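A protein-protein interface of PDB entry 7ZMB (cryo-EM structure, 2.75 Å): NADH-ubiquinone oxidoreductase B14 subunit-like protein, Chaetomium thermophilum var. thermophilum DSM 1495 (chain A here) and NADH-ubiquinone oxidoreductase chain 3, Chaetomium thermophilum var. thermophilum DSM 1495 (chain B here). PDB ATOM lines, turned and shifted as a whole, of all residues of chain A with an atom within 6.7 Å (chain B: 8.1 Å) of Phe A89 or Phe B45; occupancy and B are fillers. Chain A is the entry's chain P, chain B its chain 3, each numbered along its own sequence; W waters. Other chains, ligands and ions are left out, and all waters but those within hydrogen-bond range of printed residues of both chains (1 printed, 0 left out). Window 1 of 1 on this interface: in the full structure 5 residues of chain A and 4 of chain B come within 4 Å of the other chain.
The side-chain amide oxygen (OE1) of Gln A92 lies within hydrogen-bond range of the backbone NH (N) of His B43, at 2.9 Å.
CE of Met A42 touches CE1 of Phe B45, at 3.4 Å.
O of Met A87 touches CZ of Phe B45 (3.6 Å).
Asn A88 touches Phe B45 (O to CE2, 3.5 Å).
His B43 touches Phe A89 (O to CZ, 3.5 Å).
Phe A89 touches Ser B44.
CZ of Phe B45 touches CB of Phe A89, 3.7 Å away.
NE2 of Gln A92 touches CD1 of Phe B42, 3.6 Å away.
Hydrophobic or aromatic side chains of chain A within 4 Å of the printed part of chain B: Met A42 and Phe A89.
Of the 9 printed residues of chain B, 4 touch a printed residue of chain A.
Printed residues of chain B that touch a printed residue of chain A: Phe B42, His B43, Ser B44 and Phe B45.
Hydrophobic or aromatic side chains of chain B within 4 Å of the printed part of chain A: Phe B42, His B43 and Phe B45.
Among the printed residues, no Asp or Glu carboxylate lies within 4 Å of a Lys or Arg side-chain nitrogen of the other chain.
The backbone carbonyl oxygen (O) of Phe A89 is in hydrogen-bond range of the side-chain amide nitrogen (NE2) of Gln A92, at 3.5 Å.
ND2 of Asn A88 is in hydrogen-bond range of O of Gln A84 (2.5 Å).
Water W1 lies within hydrogen-bond range of O of Phe A89, O of His B43 and OG of Ser B44.
Glu A38 touches none of the printed residues of chain B.
Of the printed residues of chain B, Met A42 touches Phe B45.
Thr A86 touches none of the printed residues of chain B.
Of the printed residues of chain B, Met A87 touches Phe B45 (3.6 Å).
Of the printed residues of chain B, Asn A88 touches Phe B45 (3.5 Å).
Phe A89 touches three residues of chain B.
Of the printed residues of chain B, Gln A92 touches Phe B42 (3.6 Å) and His B43 (2.9 Å).
Printed residues of chain A within 4 Å of Ser B44: Phe A89 (3.5 Å).
Phe B45 touches just these residues of chain A: Met A42, Met A87, Asn A88 and Phe A89.
The nearest residue of chain A that does not touch Phe B45 is Glu A38 (6.0 Å).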
ATOM      1  N   LYS A   7      18.020  -3.571   6.152  1.00  0.00           N
ATOM      2  CA  LYS A   7      18.744  -2.382   5.719  1.00  0.00           C
ATOM      3  C   LYS A   7      18.130  -1.087   6.244  1.00  0.00           C
ATOM      4  O   LYS A   7      18.855  -0.198   6.710  1.00  0.00           O
ATOM      5  CB  LYS A   7      18.838  -2.333   4.198  1.00  0.00           C
ATOM      6  CG  LYS A   7      19.561  -1.106   3.764  1.00  0.00           C
ATOM      7  CD  LYS A   7      19.712  -0.978   2.293  1.00  0.00           C
ATOM      8  CE  LYS A   7      20.815  -1.881   1.817  1.00  0.00           C
ATOM      9  NZ  LYS A   7      21.120  -1.565   0.422  1.00  0.00           N
ATOM     10  N   GLU A  38      13.803   7.158  -7.113  1.00  0.00           N
ATOM     11  CA  GLU A  38      14.317   5.799  -6.979  1.00  0.00           C
ATOM     12  C   GLU A  38      13.195   4.770  -6.959  1.00  0.00           C
ATOM     13  O   GLU A  38      13.402   3.620  -7.360  1.00  0.00           O
ATOM     14  CB  GLU A  38      15.167   5.709  -5.720  1.00  0.00           C
ATOM     15  CG  GLU A  38      15.834   4.385  -5.486  1.00  0.00           C
ATOM     16  CD  GLU A  38      16.698   4.405  -4.250  1.00  0.00           C
ATOM     17  OE1 GLU A  38      16.743   5.454  -3.578  1.00  0.00           O
ATOM     18  OE2 GLU A  38      17.344   3.377  -3.957  1.00  0.00           O
ATOM     19  N   THR A  41      12.053   3.934 -10.910  1.00  0.00           N
ATOM     20  CA  THR A  41      12.804   2.998 -11.738  1.00  0.00           C
ATOM     21  C   THR A  41      12.853   1.611 -11.113  1.00  0.00           C
ATOM     22  O   THR A  41      13.018   0.614 -11.825  1.00  0.00           O
ATOM     23  CB  THR A  41      14.210   3.533 -11.998  1.00  0.00           C
ATOM     24  OG1 THR A  41      14.825   3.897 -10.758  1.00  0.00           O
ATOM     25  CG2 THR A  41      14.163   4.724 -12.940  1.00  0.00           C
ATOM     26  N   MET A  42      12.727   1.522  -9.790  1.00  0.00           N
ATOM     27  CA  MET A  42      12.606   0.214  -9.155  1.00  0.00           C
ATOM     28  C   MET A  42      11.334  -0.492  -9.589  1.00  0.00           C
ATOM     29  O   MET A  42      11.348  -1.692  -9.881  1.00  0.00           O
ATOM     30  CB  MET A  42      12.608   0.357  -7.640  1.00  0.00           C
ATOM     31  CG  MET A  42      12.757  -0.953  -6.896  1.00  0.00           C
ATOM     32  SD  MET A  42      12.557  -0.741  -5.120  1.00  0.00           S
ATOM     33  CE  MET A  42      14.217  -0.333  -4.641  1.00  0.00           C
ATOM     34  N   TYR A  43      10.226   0.232  -9.625  1.00  0.00           N
ATOM     35  CA  TYR A  43       8.921  -0.341  -9.895  1.00  0.00           C
ATOM     36  C   TYR A  43       8.434  -0.042 -11.302  1.00  0.00           C
ATOM     37  O   TYR A  43       7.283  -0.346 -11.621  1.00  0.00           O
ATOM     38  CB  TYR A  43       7.928   0.159  -8.852  1.00  0.00           C
ATOM     39  CG  TYR A  43       8.232  -0.410  -7.492  1.00  0.00           C
ATOM     40  CD1 TYR A  43       8.079  -1.763  -7.239  1.00  0.00           C
ATOM     41  CD2 TYR A  43       8.731   0.390  -6.482  1.00  0.00           C
ATOM     42  CE1 TYR A  43       8.378  -2.291  -6.016  1.00  0.00           C
ATOM     43  CE2 TYR A  43       9.040  -0.134  -5.254  1.00  0.00           C
ATOM     44  CZ  TYR A  43       8.861  -1.475  -5.028  1.00  0.00           C
ATOM     45  OH  TYR A  43       9.158  -1.997  -3.801  1.00  0.00           O
ATOM     46  N   GLN A  84      10.665   1.180   4.610  1.00  0.00           N
ATOM     47  CA  GLN A  84      11.609   0.073   4.580  1.00  0.00           C
ATOM     48  C   GLN A  84      11.148  -1.014   3.626  1.00  0.00           C
ATOM     49  O   GLN A  84      11.953  -1.602   2.899  1.00  0.00           O
ATOM     50  CB  GLN A  84      11.775  -0.495   5.982  1.00  0.00           C
ATOM     51  CG  GLN A  84      12.772  -1.597   6.082  1.00  0.00           C
ATOM     52  CD  GLN A  84      12.555  -2.426   7.306  1.00  0.00           C
ATOM     53  OE1 GLN A  84      11.469  -2.425   7.872  1.00  0.00           O
ATOM     54  NE2 GLN A  84      13.581  -3.142   7.728  1.00  0.00           N
ATOM     55  N   GLU A  85       9.850  -1.293   3.632  1.00  0.00           N
ATOM     56  CA  GLU A  85       9.278  -2.299   2.756  1.00  0.00           C
ATOM     57  C   GLU A  85       9.444  -1.933   1.291  1.00  0.00           C
ATOM     58  O   GLU A  85       9.723  -2.798   0.454  1.00  0.00           O
ATOM     59  CB  GLU A  85       7.814  -2.467   3.118  1.00  0.00           C
ATOM     60  CG  GLU A  85       7.097  -3.500   2.372  1.00  0.00           C
ATOM     61  CD  GLU A  85       5.682  -3.621   2.842  1.00  0.00           C
ATOM     62  OE1 GLU A  85       5.265  -2.877   3.749  1.00  0.00           O
ATOM     63  OE2 GLU A  85       4.971  -4.445   2.279  1.00  0.00           O
ATOM     64  N   THR A  86       9.267  -0.655   0.961  1.00  0.00           N
ATOM     65  CA  THR A  86       9.364  -0.192  -0.417  1.00  0.00           C
ATOM     66  C   THR A  86      10.807  -0.169  -0.917  1.00  0.00           C
ATOM     67  O   THR A  86      11.090  -0.628  -2.024  1.00  0.00           O
ATOM     68  CB  THR A  86       8.731   1.194  -0.531  1.00  0.00           C
ATOM     69  OG1 THR A  86       7.448   1.181   0.106  1.00  0.00           O
ATOM     70  CG2 THR A  86       8.580   1.609  -1.990  1.00  0.00           C
ATOM     71  N   MET A  87      11.730   0.357  -0.111  1.00  0.00           N
ATOM     72  CA  MET A  87      13.106   0.537  -0.561  1.00  0.00           C
ATOM     73  C   MET A  87      13.855  -0.779  -0.702  1.00  0.00           C
ATOM     74  O   MET A  87      14.720  -0.902  -1.573  1.00  0.00           O
ATOM     75  CB  MET A  87      13.862   1.457   0.397  1.00  0.00           C
ATOM     76  CG  MET A  87      13.297   2.859   0.621  1.00  0.00           C
ATOM     77  SD  MET A  87      13.544   4.051  -0.713  1.00  0.00           S
ATOM     78  CE  MET A  87      12.301   3.583  -1.908  1.00  0.00           C
ATOM     79  N   ASN A  88      13.572  -1.763   0.147  1.00  0.00           N
ATOM     80  CA  ASN A  88      14.214  -3.059  -0.019  1.00  0.00           C
ATOM     81  C   ASN A  88      13.579  -3.878  -1.125  1.00  0.00           C
ATOM     82  O   ASN A  88      14.076  -4.965  -1.427  1.00  0.00           O
ATOM     83  CB  ASN A  88      14.183  -3.862   1.276  1.00  0.00           C
ATOM     84  CG  ASN A  88      14.868  -3.166   2.407  1.00  0.00           C
ATOM     85  OD1 ASN A  88      16.070  -2.967   2.387  1.00  0.00           O
ATOM     86  ND2 ASN A  88      14.105  -2.789   3.405  1.00  0.00           N
ATOM     87  N   PHE A  89      12.556  -3.373  -1.811  1.00  0.00           N
ATOM     88  CA  PHE A  89      11.931  -4.076  -2.973  1.00  0.00           C
ATOM     89  C   PHE A  89      11.277  -5.394  -2.521  1.00  0.00           C
ATOM     90  O   PHE A  89      11.247  -6.351  -3.278  1.00  0.00           O
ATOM     91  CB  PHE A  89      12.975  -4.271  -4.080  1.00  0.00           C
ATOM     92  CG  PHE A  89      12.493  -4.455  -5.497  1.00  0.00           C
ATOM     93  CD1 PHE A  89      11.147  -4.571  -5.801  1.00  0.00           C
ATOM     94  CD2 PHE A  89      13.406  -4.517  -6.536  1.00  0.00           C
ATOM     95  CE1 PHE A  89      10.727  -4.746  -7.110  1.00  0.00           C
ATOM     96  CE2 PHE A  89      12.984  -4.686  -7.845  1.00  0.00           C
ATOM     97  CZ  PHE A  89      11.646  -4.798  -8.130  1.00  0.00           C
ATOM     98  N   TRP A  90      10.767  -5.451  -1.299  1.00  0.00           N
ATOM     99  CA  TRP A  90       9.989  -6.597  -0.844  1.00  0.00           C
ATOM    100  C   TRP A  90       8.611  -6.621  -1.491  1.00  0.00           C
ATOM    101  O   TRP A  90       8.145  -7.675  -1.941  1.00  0.00           O
ATOM    102  CB  TRP A  90       9.844  -6.560   0.677  1.00  0.00           C
ATOM    103  CG  TRP A  90      11.136  -6.586   1.418  1.00  0.00           C
ATOM    104  CD1 TRP A  90      12.327  -7.057   0.966  1.00  0.00           C
ATOM    105  CD2 TRP A  90      11.368  -6.124   2.750  1.00  0.00           C
ATOM    106  NE1 TRP A  90      13.284  -6.919   1.926  1.00  0.00           N
ATOM    107  CE2 TRP A  90      12.724  -6.349   3.035  1.00  0.00           C
ATOM    108  CE3 TRP A  90      10.559  -5.541   3.731  1.00  0.00           C
ATOM    109  CZ2 TRP A  90      13.294  -6.013   4.257  1.00  0.00           C
ATOM    110  CZ3 TRP A  90      11.127  -5.205   4.940  1.00  0.00           C
ATOM    111  CH2 TRP A  90      12.479  -5.445   5.195  1.00  0.00           C
ATOM    112  N   ARG A  91       7.939  -5.482  -1.528  1.00  0.00           N
ATOM    113  CA  ARG A  91       6.721  -5.409  -2.305  1.00  0.00           C
ATOM    114  C   ARG A  91       7.062  -5.314  -3.789  1.00  0.00           C
ATOM    115  O   ARG A  91       8.212  -5.120  -4.181  1.00  0.00           O
ATOM    116  CB  ARG A  91       5.857  -4.238  -1.838  1.00  0.00           C
ATOM    117  CG  ARG A  91       6.466  -2.883  -2.025  1.00  0.00           C
ATOM    118  CD  ARG A  91       5.458  -1.806  -1.708  1.00  0.00           C
ATOM    119  NE  ARG A  91       5.164  -1.670  -0.289  1.00  0.00           N
ATOM    120  CZ  ARG A  91       4.166  -0.943   0.184  1.00  0.00           C
ATOM    121  NH1 ARG A  91       3.959  -0.850   1.486  1.00  0.00           N
ATOM    122  NH2 ARG A  91       3.360  -0.321  -0.658  1.00  0.00           N
ATOM    123  N   GLN A  92       6.049  -5.536  -4.613  1.00  0.00           N
ATOM    124  CA  GLN A  92       6.281  -5.611  -6.064  1.00  0.00           C
ATOM    125  C   GLN A  92       5.465  -4.536  -6.773  1.00  0.00           C
ATOM    126  O   GLN A  92       4.841  -3.721  -6.086  1.00  0.00           O
ATOM    127  CB  GLN A  92       5.930  -7.027  -6.500  1.00  0.00           C
ATOM    128  CG  GLN A  92       6.763  -8.103  -5.821  1.00  0.00           C
ATOM    129  CD  GLN A  92       8.182  -8.109  -6.331  1.00  0.00           C
ATOM    130  OE1 GLN A  92       8.424  -8.169  -7.533  1.00  0.00           O
ATOM    131  NE2 GLN A  92       9.135  -8.054  -5.419  1.00  0.00           N
ATOM    132  N   GLN A  93       5.449  -4.562  -8.093  1.00  0.00           N
ATOM    133  CA  GLN A  93       4.806  -3.505  -8.865  1.00  0.00           C
ATOM    134  C   GLN A  93       3.308  -3.456  -8.606  1.00  0.00           C
ATOM    135  O   GLN A  93       2.730  -2.372  -8.491  1.00  0.00           O
ATOM    136  CB  GLN A  93       5.088  -3.683 -10.352  1.00  0.00           C
ATOM    137  CG  GLN A  93       4.634  -2.507 -11.183  1.00  0.00           C
ATOM    138  CD  GLN A  93       4.456  -2.853 -12.627  1.00  0.00           C
ATOM    139  OE1 GLN A  93       3.707  -3.759 -12.973  1.00  0.00           O
ATOM    140  NE2 GLN A  93       5.146  -2.125 -13.494  1.00  0.00           N
ATOM    141  N   ALA B  37      13.722 -11.606 -15.892  1.00  0.00           N
ATOM    142  CA  ALA B  37      14.668 -12.477 -15.220  1.00  0.00           C
ATOM    143  C   ALA B  37      13.940 -13.387 -14.246  1.00  0.00           C
ATOM    144  O   ALA B  37      12.922 -13.015 -13.660  1.00  0.00           O
ATOM    145  CB  ALA B  37      15.722 -11.660 -14.476  1.00  0.00           C
ATOM    146  N   GLU B  39      13.777 -14.937 -10.749  1.00  0.00           N
ATOM    147  CA  GLU B  39      14.203 -14.687  -9.381  1.00  0.00           C
ATOM    148  C   GLU B  39      13.243 -15.369  -8.410  1.00  0.00           C
ATOM    149  O   GLU B  39      12.820 -14.791  -7.405  1.00  0.00           O
ATOM    150  CB  GLU B  39      14.317 -13.182  -9.131  1.00  0.00           C
ATOM    151  CG  GLU B  39      14.806 -12.754  -7.752  1.00  0.00           C
ATOM    152  CD  GLU B  39      16.204 -13.181  -7.416  1.00  0.00           C
ATOM    153  OE1 GLU B  39      16.436 -14.367  -7.118  1.00  0.00           O
ATOM    154  OE2 GLU B  39      17.053 -12.295  -7.357  1.00  0.00           O
ATOM    155  N   PHE B  42       9.735 -13.367  -7.556  1.00  0.00           N
ATOM    156  CA  PHE B  42       9.749 -11.970  -7.153  1.00  0.00           C
ATOM    157  C   PHE B  42      10.813 -11.232  -7.946  1.00  0.00           C
ATOM    158  O   PHE B  42      11.904 -11.757  -8.156  1.00  0.00           O
ATOM    159  CB  PHE B  42      10.032 -11.827  -5.661  1.00  0.00           C
ATOM    160  CG  PHE B  42       8.891 -12.217  -4.793  1.00  0.00           C
ATOM    161  CD1 PHE B  42       7.907 -11.305  -4.482  1.00  0.00           C
ATOM    162  CD2 PHE B  42       8.797 -13.497  -4.286  1.00  0.00           C
ATOM    163  CE1 PHE B  42       6.858 -11.658  -3.682  1.00  0.00           C
ATOM    164  CE2 PHE B  42       7.749 -13.854  -3.491  1.00  0.00           C
ATOM    165  CZ  PHE B  42       6.779 -12.935  -3.188  1.00  0.00           C
ATOM    166  N   HIS B  43      10.495 -10.036  -8.456  1.00  0.00           N
ATOM    167  CA  HIS B  43      11.514  -9.219  -9.184  1.00  0.00           C
ATOM    168  C   HIS B  43      12.455  -8.600  -8.162  1.00  0.00           C
ATOM    169  O   HIS B  43      11.972  -8.102  -7.144  1.00  0.00           O
ATOM    170  CB  HIS B  43      10.892  -8.098 -10.011  1.00  0.00           C
ATOM    171  CG  HIS B  43      10.151  -8.555 -11.216  1.00  0.00           C
ATOM    172  ND1 HIS B  43      10.733  -9.350 -12.178  1.00  0.00           N
ATOM    173  CD2 HIS B  43       8.894  -8.305 -11.636  1.00  0.00           C
ATOM    174  CE1 HIS B  43       9.859  -9.584 -13.132  1.00  0.00           C
ATOM    175  NE2 HIS B  43       8.726  -8.953 -12.825  1.00  0.00           N
ATOM    176  N   SER B  44      13.755  -8.661  -8.415  1.00  0.00           N
ATOM    177  CA  SER B  44      14.687  -8.004  -7.474  1.00  0.00           C
ATOM    178  C   SER B  44      15.586  -7.005  -8.176  1.00  0.00           C
ATOM    179  O   SER B  44      15.353  -6.725  -9.359  1.00  0.00           O
ATOM    180  CB  SER B  44      15.495  -9.008  -6.699  1.00  0.00           C
ATOM    181  OG  SER B  44      16.113  -8.410  -5.571  1.00  0.00           O
ATOM    182  N   PHE B  45      16.563  -6.488  -7.447  1.00  0.00           N
ATOM    183  CA  PHE B  45      17.575  -5.604  -8.007  1.00  0.00           C
ATOM    184  C   PHE B  45      18.353  -6.316  -9.102  1.00  0.00           C
ATOM    185  O   PHE B  45      18.764  -7.465  -8.935  1.00  0.00           O
ATOM    186  CB  PHE B  45      18.523  -5.152  -6.901  1.00  0.00           C
ATOM    187  CG  PHE B  45      17.837  -4.493  -5.752  1.00  0.00           C
ATOM    188  CD1 PHE B  45      17.478  -3.163  -5.818  1.00  0.00           C
ATOM    189  CD2 PHE B  45      17.521  -5.211  -4.614  1.00  0.00           C
ATOM    190  CE1 PHE B  45      16.842  -2.559  -4.770  1.00  0.00           C
ATOM    191  CE2 PHE B  45      16.875  -4.613  -3.561  1.00  0.00           C
ATOM    192  CZ  PHE B  45      16.537  -3.284  -3.636  1.00  0.00           C
ATOM    193  N   SER B  46      18.562  -5.635 -10.224  1.00  0.00           N
ATOM    194  CA  SER B  46      19.381  -6.174 -11.309  1.00  0.00           C
ATOM    195  C   SER B  46      20.821  -5.745 -11.059  1.00  0.00           C
ATOM    196  O   SER B  46      21.190  -4.591 -11.282  1.00  0.00           O
ATOM    197  CB  SER B  46      18.874  -5.696 -12.662  1.00  0.00           C
ATOM    198  OG  SER B  46      19.675  -6.212 -13.706  1.00  0.00           O
ATOM    199  N   GLN B  47      21.632  -6.675 -10.565  1.00  0.00           N
ATOM    200  CA  GLN B  47      22.987  -6.379 -10.121  1.00  0.00           C
ATOM    201  C   GLN B  47      23.968  -7.485 -10.487  1.00  0.00           C
ATOM    202  O   GLN B  47      24.933  -7.733  -9.769  1.00  0.00           O
ATOM    203  CB  GLN B  47      22.972  -6.061  -8.629  1.00  0.00           C
ATOM    204  CG  GLN B  47      22.546  -7.208  -7.787  1.00  0.00           C
ATOM    205  CD  GLN B  47      22.458  -6.876  -6.333  1.00  0.00           C
ATOM    206  OE1 GLN B  47      22.774  -5.776  -5.899  1.00  0.00           O
ATOM    207  NE2 GLN B  47      21.915  -7.796  -5.585  1.00  0.00           N
ATOM    208  N   SER B  48      23.737  -8.143 -11.620  1.00  0.00           N
ATOM    209  CA  SER B  48      24.643  -9.137 -12.178  1.00  0.00           C
ATOM    210  C   SER B  48      25.655  -8.533 -13.144  1.00  0.00           C
ATOM    211  O   SER B  48      26.496  -9.261 -13.675  1.00  0.00           O
ATOM    212  CB  SER B  48      23.846 -10.229 -12.896  1.00  0.00           C
ATOM    213  OG  SER B  48      23.328 -11.182 -11.989  1.00  0.00           O
HETATM  214  O   HOH W   1      12.874  -7.995  -4.615  1.00  0.00           O
